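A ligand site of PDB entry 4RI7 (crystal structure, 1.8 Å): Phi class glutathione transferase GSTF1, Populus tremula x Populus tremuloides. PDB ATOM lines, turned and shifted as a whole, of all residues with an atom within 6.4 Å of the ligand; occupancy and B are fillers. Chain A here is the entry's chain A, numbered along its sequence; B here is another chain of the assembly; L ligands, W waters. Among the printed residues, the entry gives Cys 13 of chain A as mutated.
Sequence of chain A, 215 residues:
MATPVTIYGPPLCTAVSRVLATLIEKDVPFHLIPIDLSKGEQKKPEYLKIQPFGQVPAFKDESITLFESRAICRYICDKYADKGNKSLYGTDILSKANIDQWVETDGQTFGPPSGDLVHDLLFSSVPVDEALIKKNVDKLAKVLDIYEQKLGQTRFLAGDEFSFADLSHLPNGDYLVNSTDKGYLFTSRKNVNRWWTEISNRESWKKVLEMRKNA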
ATOM      1  N   LEU A  12      12.977 -11.604  10.397  1.00  0.00           N
ATOM      2  CA  LEU A  12      13.898 -11.160   9.365  1.00  0.00           C
ATOM      3  C   LEU A  12      13.133 -10.933   8.057  1.00  0.00           C
ATOM      4  O   LEU A  12      13.600 -10.195   7.193  1.00  0.00           O
ATOM      5  CB  LEU A  12      15.027 -12.150   9.163  1.00  0.00           C
ATOM      6  CG  LEU A  12      14.679 -13.495   8.567  1.00  0.00           C
ATOM      7  CD1 LEU A  12      14.674 -13.470   7.026  1.00  0.00           C
ATOM      8  CD2 LEU A  12      15.663 -14.562   9.091  1.00  0.00           C
ATOM      9  N   CYS A  13      11.971 -11.558   7.924  1.00  0.00           N
ATOM     10  CA  CYS A  13      11.089 -11.343   6.782  1.00  0.00           C
ATOM     11  C   CYS A  13      10.446  -9.956   6.824  1.00  0.00           C
ATOM     12  O   CYS A  13       9.818  -9.557   7.833  1.00  0.00           O
ATOM     13  CB  CYS A  13      10.017 -12.421   6.733  1.00  0.00           C
ATOM     14  SG  CYS A  13       8.676 -12.003   5.589  1.00  0.00           S
ATOM     15  N   THR A  14      10.620  -9.204   5.733  1.00  0.00           N
ATOM     16  CA  THR A  14      10.143  -7.840   5.644  1.00  0.00           C
ATOM     17  C   THR A  14       8.623  -7.758   5.891  1.00  0.00           C
ATOM     18  O   THR A  14       8.166  -6.839   6.500  1.00  0.00           O
ATOM     19  CB  THR A  14      10.412  -7.198   4.273  1.00  0.00           C
ATOM     20  OG1 THR A  14       9.940  -8.082   3.253  1.00  0.00           O
ATOM     21  CG2 THR A  14      11.915  -6.882   4.066  1.00  0.00           C
ATOM     22  N   ALA A  15       7.873  -8.709   5.363  1.00  0.00           N
ATOM     23  CA  ALA A  15       6.413  -8.679   5.452  1.00  0.00           C
ATOM     24  C   ALA A  15       5.962  -9.022   6.887  1.00  0.00           C
ATOM     25  O   ALA A  15       4.992  -8.463   7.374  1.00  0.00           O
ATOM     26  CB  ALA A  15       5.785  -9.642   4.444  1.00  0.00           C
ATOM     27  N   VAL A  16       6.691  -9.944   7.525  1.00  0.00           N
ATOM     28  CA  VAL A  16       6.489 -10.236   8.937  1.00  0.00           C
ATOM     29  C   VAL A  16       6.814  -8.981   9.780  1.00  0.00           C
ATOM     30  O   VAL A  16       6.076  -8.618  10.715  1.00  0.00           O
ATOM     31  CB  VAL A  16       7.353 -11.438   9.411  1.00  0.00           C
ATOM     32  CG1 VAL A  16       7.264 -11.606  10.915  1.00  0.00           C
ATOM     33  CG2 VAL A  16       6.953 -12.762   8.721  1.00  0.00           C
ATOM     34  N   ARG A  18       6.623  -5.893   8.926  1.00  0.00           N
ATOM     35  CA  ARG A  18       5.539  -4.926   8.779  1.00  0.00           C
ATOM     36  C   ARG A  18       4.431  -5.211   9.782  1.00  0.00           C
ATOM     37  O   ARG A  18       3.956  -4.320  10.486  1.00  0.00           O
ATOM     38  CB  ARG A  18       5.015  -4.943   7.347  1.00  0.00           C
ATOM     39  CG  ARG A  18       3.789  -4.062   7.123  1.00  0.00           C
ATOM     40  CD  ARG A  18       3.341  -4.118   5.636  1.00  0.00           C
ATOM     41  NE  ARG A  18       4.382  -3.543   4.777  1.00  0.00           N
ATOM     42  CZ  ARG A  18       5.275  -4.204   4.048  1.00  0.00           C
ATOM     43  NH1 ARG A  18       5.289  -5.532   3.948  1.00  0.00           N
ATOM     44  NH2 ARG A  18       6.168  -3.499   3.376  1.00  0.00           N
ATOM     45  N   LEU A  37      12.339 -20.293   6.857  1.00  0.00           N
ATOM     46  CA  LEU A  37      12.378 -20.197   5.400  1.00  0.00           C
ATOM     47  C   LEU A  37      13.622 -20.856   4.803  1.00  0.00           C
ATOM     48  O   LEU A  37      13.608 -21.283   3.633  1.00  0.00           O
ATOM     49  CB  LEU A  37      12.320 -18.739   4.959  1.00  0.00           C
ATOM     50  CG  LEU A  37      11.081 -17.952   5.428  1.00  0.00           C
ATOM     51  CD1 LEU A  37      11.088 -16.555   4.793  1.00  0.00           C
ATOM     52  CD2 LEU A  37       9.753 -18.696   5.128  1.00  0.00           C
ATOM     53  N   GLN A  42       7.639 -23.166   5.166  1.00  0.00           N
ATOM     54  CA  GLN A  42       6.460 -22.476   4.639  1.00  0.00           C
ATOM     55  C   GLN A  42       5.714 -23.281   3.571  1.00  0.00           C
ATOM     56  O   GLN A  42       4.613 -22.900   3.142  1.00  0.00           O
ATOM     57  CB  GLN A  42       6.860 -21.114   4.043  1.00  0.00           C
ATOM     58  CG  GLN A  42       7.649 -21.186   2.704  1.00  0.00           C
ATOM     59  CD  GLN A  42       9.119 -21.521   2.879  1.00  0.00           C
ATOM     60  OE1 GLN A  42       9.536 -22.097   3.877  1.00  0.00           O
ATOM     61  NE2 GLN A  42       9.924 -21.123   1.890  1.00  0.00           N
ATOM     62  N   LYS A  43       6.336 -24.364   3.104  1.00  0.00           N
ATOM     63  CA  LYS A  43       5.780 -25.195   2.036  1.00  0.00           C
ATOM     64  C   LYS A  43       5.188 -26.503   2.544  1.00  0.00           C
ATOM     65  O   LYS A  43       4.643 -27.270   1.766  1.00  0.00           O
ATOM     66  CB  LYS A  43       6.860 -25.515   0.985  1.00  0.00           C
ATOM     67  CG  LYS A  43       7.485 -24.287   0.344  1.00  0.00           C
ATOM     68  CD  LYS A  43       6.411 -23.372  -0.253  1.00  0.00           C
ATOM     69  CE  LYS A  43       7.018 -22.202  -1.043  1.00  0.00           C
ATOM     70  NZ  LYS A  43       5.973 -21.172  -1.410  1.00  0.00           N
ATOM     71  N   GLN A  51      -1.749 -20.443   4.781  1.00  0.00           N
ATOM     72  CA  GLN A  51      -1.305 -19.443   3.817  1.00  0.00           C
ATOM     73  C   GLN A  51      -1.122 -20.139   2.469  1.00  0.00           C
ATOM     74  O   GLN A  51      -0.134 -20.830   2.240  1.00  0.00           O
ATOM     75  CB  GLN A  51      -0.021 -18.755   4.313  1.00  0.00           C
ATOM     76  CG  GLN A  51       0.049 -17.265   3.968  1.00  0.00           C
ATOM     77  CD  GLN A  51       0.476 -17.004   2.534  1.00  0.00           C
ATOM     78  OE1 GLN A  51       0.503 -17.920   1.710  1.00  0.00           O
ATOM     79  NE2 GLN A  51       0.845 -15.764   2.232  1.00  0.00           N
ATOM     80  N   PHE A  53      -0.386 -19.569  -0.493  1.00  0.00           N
ATOM     81  CA  PHE A  53       0.754 -19.282  -1.343  1.00  0.00           C
ATOM     82  C   PHE A  53       2.096 -19.759  -0.747  1.00  0.00           C
ATOM     83  O   PHE A  53       3.143 -19.690  -1.413  1.00  0.00           O
ATOM     84  CB  PHE A  53       0.782 -17.779  -1.649  1.00  0.00           C
ATOM     85  CG  PHE A  53      -0.407 -17.322  -2.421  1.00  0.00           C
ATOM     86  CD1 PHE A  53      -0.426 -17.414  -3.815  1.00  0.00           C
ATOM     87  CD2 PHE A  53      -1.558 -16.874  -1.773  1.00  0.00           C
ATOM     88  CE1 PHE A  53      -1.539 -17.030  -4.528  1.00  0.00           C
ATOM     89  CE2 PHE A  53      -2.668 -16.476  -2.486  1.00  0.00           C
ATOM     90  CZ  PHE A  53      -2.667 -16.581  -3.871  1.00  0.00           C
ATOM     91  N   GLY A  54       2.077 -20.303   0.467  1.00  0.00           N
ATOM     92  CA  GLY A  54       3.300 -20.842   1.048  1.00  0.00           C
ATOM     93  C   GLY A  54       4.271 -19.740   1.400  1.00  0.00           C
ATOM     94  O   GLY A  54       5.479 -19.874   1.259  1.00  0.00           O
ATOM     95  N   GLN A  55       3.716 -18.619   1.836  1.00  0.00           N
ATOM     96  CA  GLN A  55       4.516 -17.480   2.249  1.00  0.00           C
ATOM     97  C   GLN A  55       4.165 -17.064   3.649  1.00  0.00           C
ATOM     98  O   GLN A  55       3.120 -17.447   4.185  1.00  0.00           O
ATOM     99  CB  GLN A  55       4.319 -16.304   1.293  1.00  0.00           C
ATOM    100  CG  GLN A  55       4.704 -16.657  -0.123  1.00  0.00           C
ATOM    101  CD  GLN A  55       4.914 -15.422  -0.981  1.00  0.00           C
ATOM    102  OE1 GLN A  55       4.009 -14.605  -1.157  1.00  0.00           O
ATOM    103  NE2 GLN A  55       6.127 -15.273  -1.498  1.00  0.00           N
ATOM    104  N   VAL A  56       5.061 -16.295   4.245  1.00  0.00           N
ATOM    105  CA  VAL A  56       4.826 -15.680   5.552  1.00  0.00           C
ATOM    106  C   VAL A  56       4.707 -14.160   5.340  1.00  0.00           C
ATOM    107  O   VAL A  56       5.243 -13.622   4.407  1.00  0.00           O
ATOM    108  CB  VAL A  56       5.968 -16.013   6.546  1.00  0.00           C
ATOM    109  CG1 VAL A  56       5.965 -17.502   6.843  1.00  0.00           C
ATOM    110  CG2 VAL A  56       7.306 -15.644   5.981  1.00  0.00           C
ATOM    111  N   PRO A  57       3.999 -13.461   6.221  1.00  0.00           N
ATOM    112  CA  PRO A  57       3.308 -13.894   7.418  1.00  0.00           C
ATOM    113  C   PRO A  57       1.914 -14.416   7.197  1.00  0.00           C
ATOM    114  O   PRO A  57       1.318 -14.216   6.154  1.00  0.00           O
ATOM    115  CB  PRO A  57       3.234 -12.602   8.245  1.00  0.00           C
ATOM    116  CG  PRO A  57       3.077 -11.536   7.220  1.00  0.00           C
ATOM    117  CD  PRO A  57       3.935 -12.000   6.043  1.00  0.00           C
ATOM    118  N   PHE A  67      -4.003 -13.532   5.566  1.00  0.00           N
ATOM    119  CA  PHE A  67      -2.640 -13.360   5.066  1.00  0.00           C
ATOM    120  C   PHE A  67      -2.543 -12.077   4.221  1.00  0.00           C
ATOM    121  O   PHE A  67      -3.514 -11.349   4.111  1.00  0.00           O
ATOM    122  CB  PHE A  67      -2.213 -14.608   4.284  1.00  0.00           C
ATOM    123  CG  PHE A  67      -3.082 -14.900   3.089  1.00  0.00           C
ATOM    124  CD1 PHE A  67      -4.222 -15.672   3.208  1.00  0.00           C
ATOM    125  CD2 PHE A  67      -2.744 -14.400   1.825  1.00  0.00           C
ATOM    126  CE1 PHE A  67      -5.039 -15.933   2.089  1.00  0.00           C
ATOM    127  CE2 PHE A  67      -3.567 -14.667   0.701  1.00  0.00           C
ATOM    128  CZ  PHE A  67      -4.708 -15.424   0.844  1.00  0.00           C
ATOM    129  N   GLU A  68      -1.371 -11.843   3.646  1.00  0.00           N
ATOM    130  CA  GLU A  68      -0.953 -10.544   3.077  1.00  0.00           C
ATOM    131  C   GLU A  68      -0.758  -9.480   4.161  1.00  0.00           C
ATOM    132  O   GLU A  68      -1.707  -9.026   4.796  1.00  0.00           O
ATOM    133  CB  GLU A  68      -1.931 -10.040   2.018  1.00  0.00           C
ATOM    134  CG  GLU A  68      -1.690 -10.739   0.658  1.00  0.00           C
ATOM    135  CD  GLU A  68      -0.394 -10.316  -0.030  1.00  0.00           C
ATOM    136  OE1 GLU A  68       0.287  -9.362   0.425  1.00  0.00           O
ATOM    137  OE2 GLU A  68      -0.066 -10.936  -1.057  1.00  0.00           O
ATOM    138  N   SER A  69       0.486  -9.084   4.340  1.00  0.00           N
ATOM    139  CA  SER A  69       0.869  -8.250   5.493  1.00  0.00           C
ATOM    140  C   SER A  69       0.032  -6.974   5.592  1.00  0.00           C
ATOM    141  O   SER A  69      -0.370  -6.617   6.690  1.00  0.00           O
ATOM    142  CB  SER A  69       2.367  -7.915   5.409  1.00  0.00           C
ATOM    143  OG  SER A  69       2.676  -7.236   4.202  1.00  0.00           O
ATOM    144  N   ARG A  70      -0.285  -6.328   4.467  1.00  0.00           N
ATOM    145  CA  ARG A  70      -0.995  -5.046   4.533  1.00  0.00           C
ATOM    146  C   ARG A  70      -2.474  -5.231   4.901  1.00  0.00           C
ATOM    147  O   ARG A  70      -3.080  -4.362   5.562  1.00  0.00           O
ATOM    148  CB  ARG A  70      -0.877  -4.269   3.211  1.00  0.00           C
ATOM    149  CG  ARG A  70       0.526  -3.711   2.965  1.00  0.00           C
ATOM    150  CD  ARG A  70       0.728  -3.279   1.519  1.00  0.00           C
ATOM    151  NE  ARG A  70       2.149  -2.977   1.275  1.00  0.00           N
ATOM    152  CZ  ARG A  70       3.067  -3.900   0.978  1.00  0.00           C
ATOM    153  NH1 ARG A  70       2.762  -5.177   0.882  1.00  0.00           N
ATOM    154  NH2 ARG A  70       4.318  -3.539   0.772  1.00  0.00           N
ATOM    155  N   ILE A  72      -3.462  -7.815   6.773  1.00  0.00           N
ATOM    156  CA  ILE A  72      -3.350  -8.134   8.182  1.00  0.00           C
ATOM    157  C   ILE A  72      -3.305  -6.826   8.995  1.00  0.00           C
ATOM    158  O   ILE A  72      -3.974  -6.703  10.024  1.00  0.00           O
ATOM    159  CB  ILE A  72      -2.119  -8.992   8.492  1.00  0.00           C
ATOM    160  CG1 ILE A  72      -2.292 -10.410   7.926  1.00  0.00           C
ATOM    161  CG2 ILE A  72      -1.865  -9.078   9.973  1.00  0.00           C
ATOM    162  CD1 ILE A  72      -0.993 -11.210   7.886  1.00  0.00           C
ATOM    163  N   GLU B 104      -5.137  -7.597  -1.689  1.00  0.00           N
ATOM    164  CA  GLU B 104      -3.674  -7.571  -1.585  1.00  0.00           C
ATOM    165  C   GLU B 104      -3.019  -8.661  -2.463  1.00  0.00           C
ATOM    166  O   GLU B 104      -1.953  -8.439  -3.026  1.00  0.00           O
ATOM    167  CB  GLU B 104      -3.244  -7.732  -0.132  1.00  0.00           C
ATOM    168  CG  GLU B 104      -3.500  -6.489   0.728  1.00  0.00           C
ATOM    169  CD  GLU B 104      -2.699  -5.279   0.235  1.00  0.00           C
ATOM    170  OE1 GLU B 104      -1.490  -5.432  -0.063  1.00  0.00           O
ATOM    171  OE2 GLU B 104      -3.261  -4.178   0.131  1.00  0.00           O
ATOM    172  N   GLN B 108      -0.115  -7.762  -4.992  1.00  0.00           N
ATOM    173  CA  GLN B 108       1.234  -8.206  -4.698  1.00  0.00           C
ATOM    174  C   GLN B 108       1.592  -9.484  -5.437  1.00  0.00           C
ATOM    175  O   GLN B 108       2.768  -9.750  -5.627  1.00  0.00           O
ATOM    176  CB  GLN B 108       1.418  -8.440  -3.181  1.00  0.00           C
ATOM    177  CG  GLN B 108       1.292  -7.199  -2.348  1.00  0.00           C
ATOM    178  CD  GLN B 108       2.225  -6.094  -2.800  1.00  0.00           C
ATOM    179  OE1 GLN B 108       3.435  -6.293  -2.871  1.00  0.00           O
ATOM    180  NE2 GLN B 108       1.664  -4.910  -3.095  1.00  0.00           N
ATOM    181  N   THR B 109       0.603 -10.278  -5.825  1.00  0.00           N
ATOM    182  CA  THR B 109       0.881 -11.630  -6.340  1.00  0.00           C
ATOM    183  C   THR B 109       0.445 -11.828  -7.766  1.00  0.00           C
ATOM    184  O   THR B 109       1.257 -12.232  -8.594  1.00  0.00           O
ATOM    185  CB  THR B 109       0.250 -12.634  -5.423  1.00  0.00           C
ATOM    186  OG1 THR B 109       0.801 -12.422  -4.104  1.00  0.00           O
ATOM    187  CG2 THR B 109       0.542 -14.069  -5.865  1.00  0.00           C
HETATM  188  N1  LIG L   1       2.749 -10.031  -0.300  1.00  0.00           N
HETATM  189  C1  LIG L   1       3.169 -10.871   0.806  1.00  0.00           C
HETATM  190  C2  LIG L   1       2.917 -10.111   2.075  1.00  0.00           C
HETATM  191  O1  LIG L   1       2.418 -10.726   3.043  1.00  0.00           O
HETATM  192  O2  LIG L   1       3.152  -8.890   2.085  1.00  0.00           O
HETATM  193  C3  LIG L   1       4.654 -11.182   0.660  1.00  0.00           C
HETATM  194  C4  LIG L   1       5.142 -12.237   1.657  1.00  0.00           C
HETATM  195  C5  LIG L   1       6.542 -12.691   1.305  1.00  0.00           C
HETATM  196  O3  LIG L   1       7.136 -12.215   0.365  1.00  0.00           O
HETATM  197  N2  LIG L   1       7.096 -13.609   2.086  1.00  0.00           N
HETATM  198  C6  LIG L   1       8.434 -14.122   1.898  1.00  0.00           C
HETATM  199  C7  LIG L   1       8.274 -15.602   1.876  1.00  0.00           C
HETATM  200  O4  LIG L   1       7.374 -16.091   2.556  1.00  0.00           O
HETATM  201  C8  LIG L   1       9.441 -13.815   2.994  1.00  0.00           C
HETATM  202  S1  LIG L   1       9.507 -12.105   3.616  1.00  0.00           S
HETATM  203  N3  LIG L   1       9.138 -16.300   1.144  1.00  0.00           N
HETATM  204  C9  LIG L   1       9.109 -17.759   1.148  1.00  0.00           C
HETATM  205  C10 LIG L   1       8.688 -18.284  -0.195  1.00  0.00           C
HETATM  206  O5  LIG L   1       8.713 -19.521  -0.388  1.00  0.00           O
HETATM  207  O6  LIG L   1       8.334 -17.458  -1.077  1.00  0.00           O
HETATM  208  O   HOH W   1       6.854 -18.587  -2.827  1.00  0.00           O
HETATM  209  O   HOH W   2       8.253  -9.652   0.716  1.00  0.00           O
HETATM  210  O   HOH W   3       5.042  -7.133   0.779  1.00  0.00           O
HETATM  211  O   HOH W   4       3.096 -11.987  -2.690  1.00  0.00           O
HETATM  212  O   HOH W   5      10.463 -20.767  -2.359  1.00  0.00           O
HETATM  213  O   HOH W   6       1.168 -13.154   3.761  1.00  0.00           O
HETATM  214  O   HOH W   7       4.718  -8.346  -1.454  1.00  0.00           O
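The side-chain sulfur (SG) of Cys 13 sits close to the backbone NH (N) of Ala 15. SG of Cys 13 is in hydrogen-bond range of N of Val 16 (3.5 Å). OE2 of Glu 68 sits at hydrogen-bond distance from OG1 of Thr 109 of chain B, at 3.5 Å. OG of Ser 69 lies within hydrogen-bond range of NH1 of Arg 18, at 3.1 Å. N of Gln 55 sits at hydrogen-bond distance from OE1 of Gln 51, at 3.3 Å. The backbone carbonyl oxygen (O) of Gly 54 is in hydrogen-bond range of the side-chain amino group (NZ) of Lys 43 (3.0 Å). NZ of Lys 43 lies within hydrogen-bond range of O of Phe 53, 3.2 Å away. The side-chain amide oxygen (OE1) of Gln 51 is in hydrogen-bond range of the backbone NH (N) of Gly 54, 3.1 Å away.
Merely in contact with the ligand: Ala 15 (3.6 Å), Leu 37 (3.7 Å), Gly 54 (3.6 Å), Pro 57 (3.6 Å) and Gln 108 of chain B (3.6 Å). 14 residues have an atom within 4 Å of the ligand: Cys 13, Thr 14, Ala 15, Leu 37, Gln 42, Lys 43, Gly 54, Gln 55, Val 56, Pro 57, Glu 68, Ser 69, Arg 70 and Gln 108 of chain B.
Water W1 bridges an oxygen (O6) of the ligand (2.6 Å) and the side-chain amino group of Lys 43 (3.1 Å). Water W2 lies within hydrogen-bond range of O3 of the ligand (2.8 Å) and OG1 of Thr 14 (3.4 Å). Water W6 lies within hydrogen-bond range of O of Pro 57 (2.6 Å), O1 of the ligand (2.8 Å), N of Glu 68 (2.9 Å) and NE2 of Gln 51 (3.0 Å). Water W7 bridges OE1 of Gln 108 of chain B (2.8 Å) and N1 of the ligand (2.8 Å). Water W3 bridges an oxygen (O2) of the ligand (2.9 Å) and the guanidinium group of Arg 70 (3.0 Å). Water W4 lies within hydrogen-bond range of OG1 of Thr 109 of chain B, N1 of the ligand and OE1 of Gln 55.
S1 of the ligand is covalently linked to SG of Cys 13 (2.1 Å). The side-chain carboxylate (OE1) of Glu 68 lies within salt-bridge range of a nitrogen (N1) of the ligand. N of Ser 69 sits at hydrogen-bond distance from O1 of the ligand, at 2.8 Å. OG of Ser 69 lies within hydrogen-bond range of O2 of the ligand, 2.7 Å away. An oxygen (O4) of the ligand sits at hydrogen-bond distance from the backbone NH (N) of Val 56 (2.9 Å). O of Val 56 lies within hydrogen-bond range of N2 of the ligand (3.0 Å). O5 of the ligand is in hydrogen-bond range of NE2 of Gln 42. An oxygen (O6) of the ligand lies within hydrogen-bond range of the side-chain amide nitrogen (NE2) of Gln 55 (3.1 Å). The side-chain amino group (NZ) of Lys 43 is in salt-bridge range of an oxygen (O5) of the ligand (3.4 Å). The backbone NH of Thr 14 lies close to a sulfur (S1) of the ligand. The guanidinium group (NH1) of Arg 70 lies within salt-bridge range of an oxygen (O2) of the ligand, 3.9 Å away.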
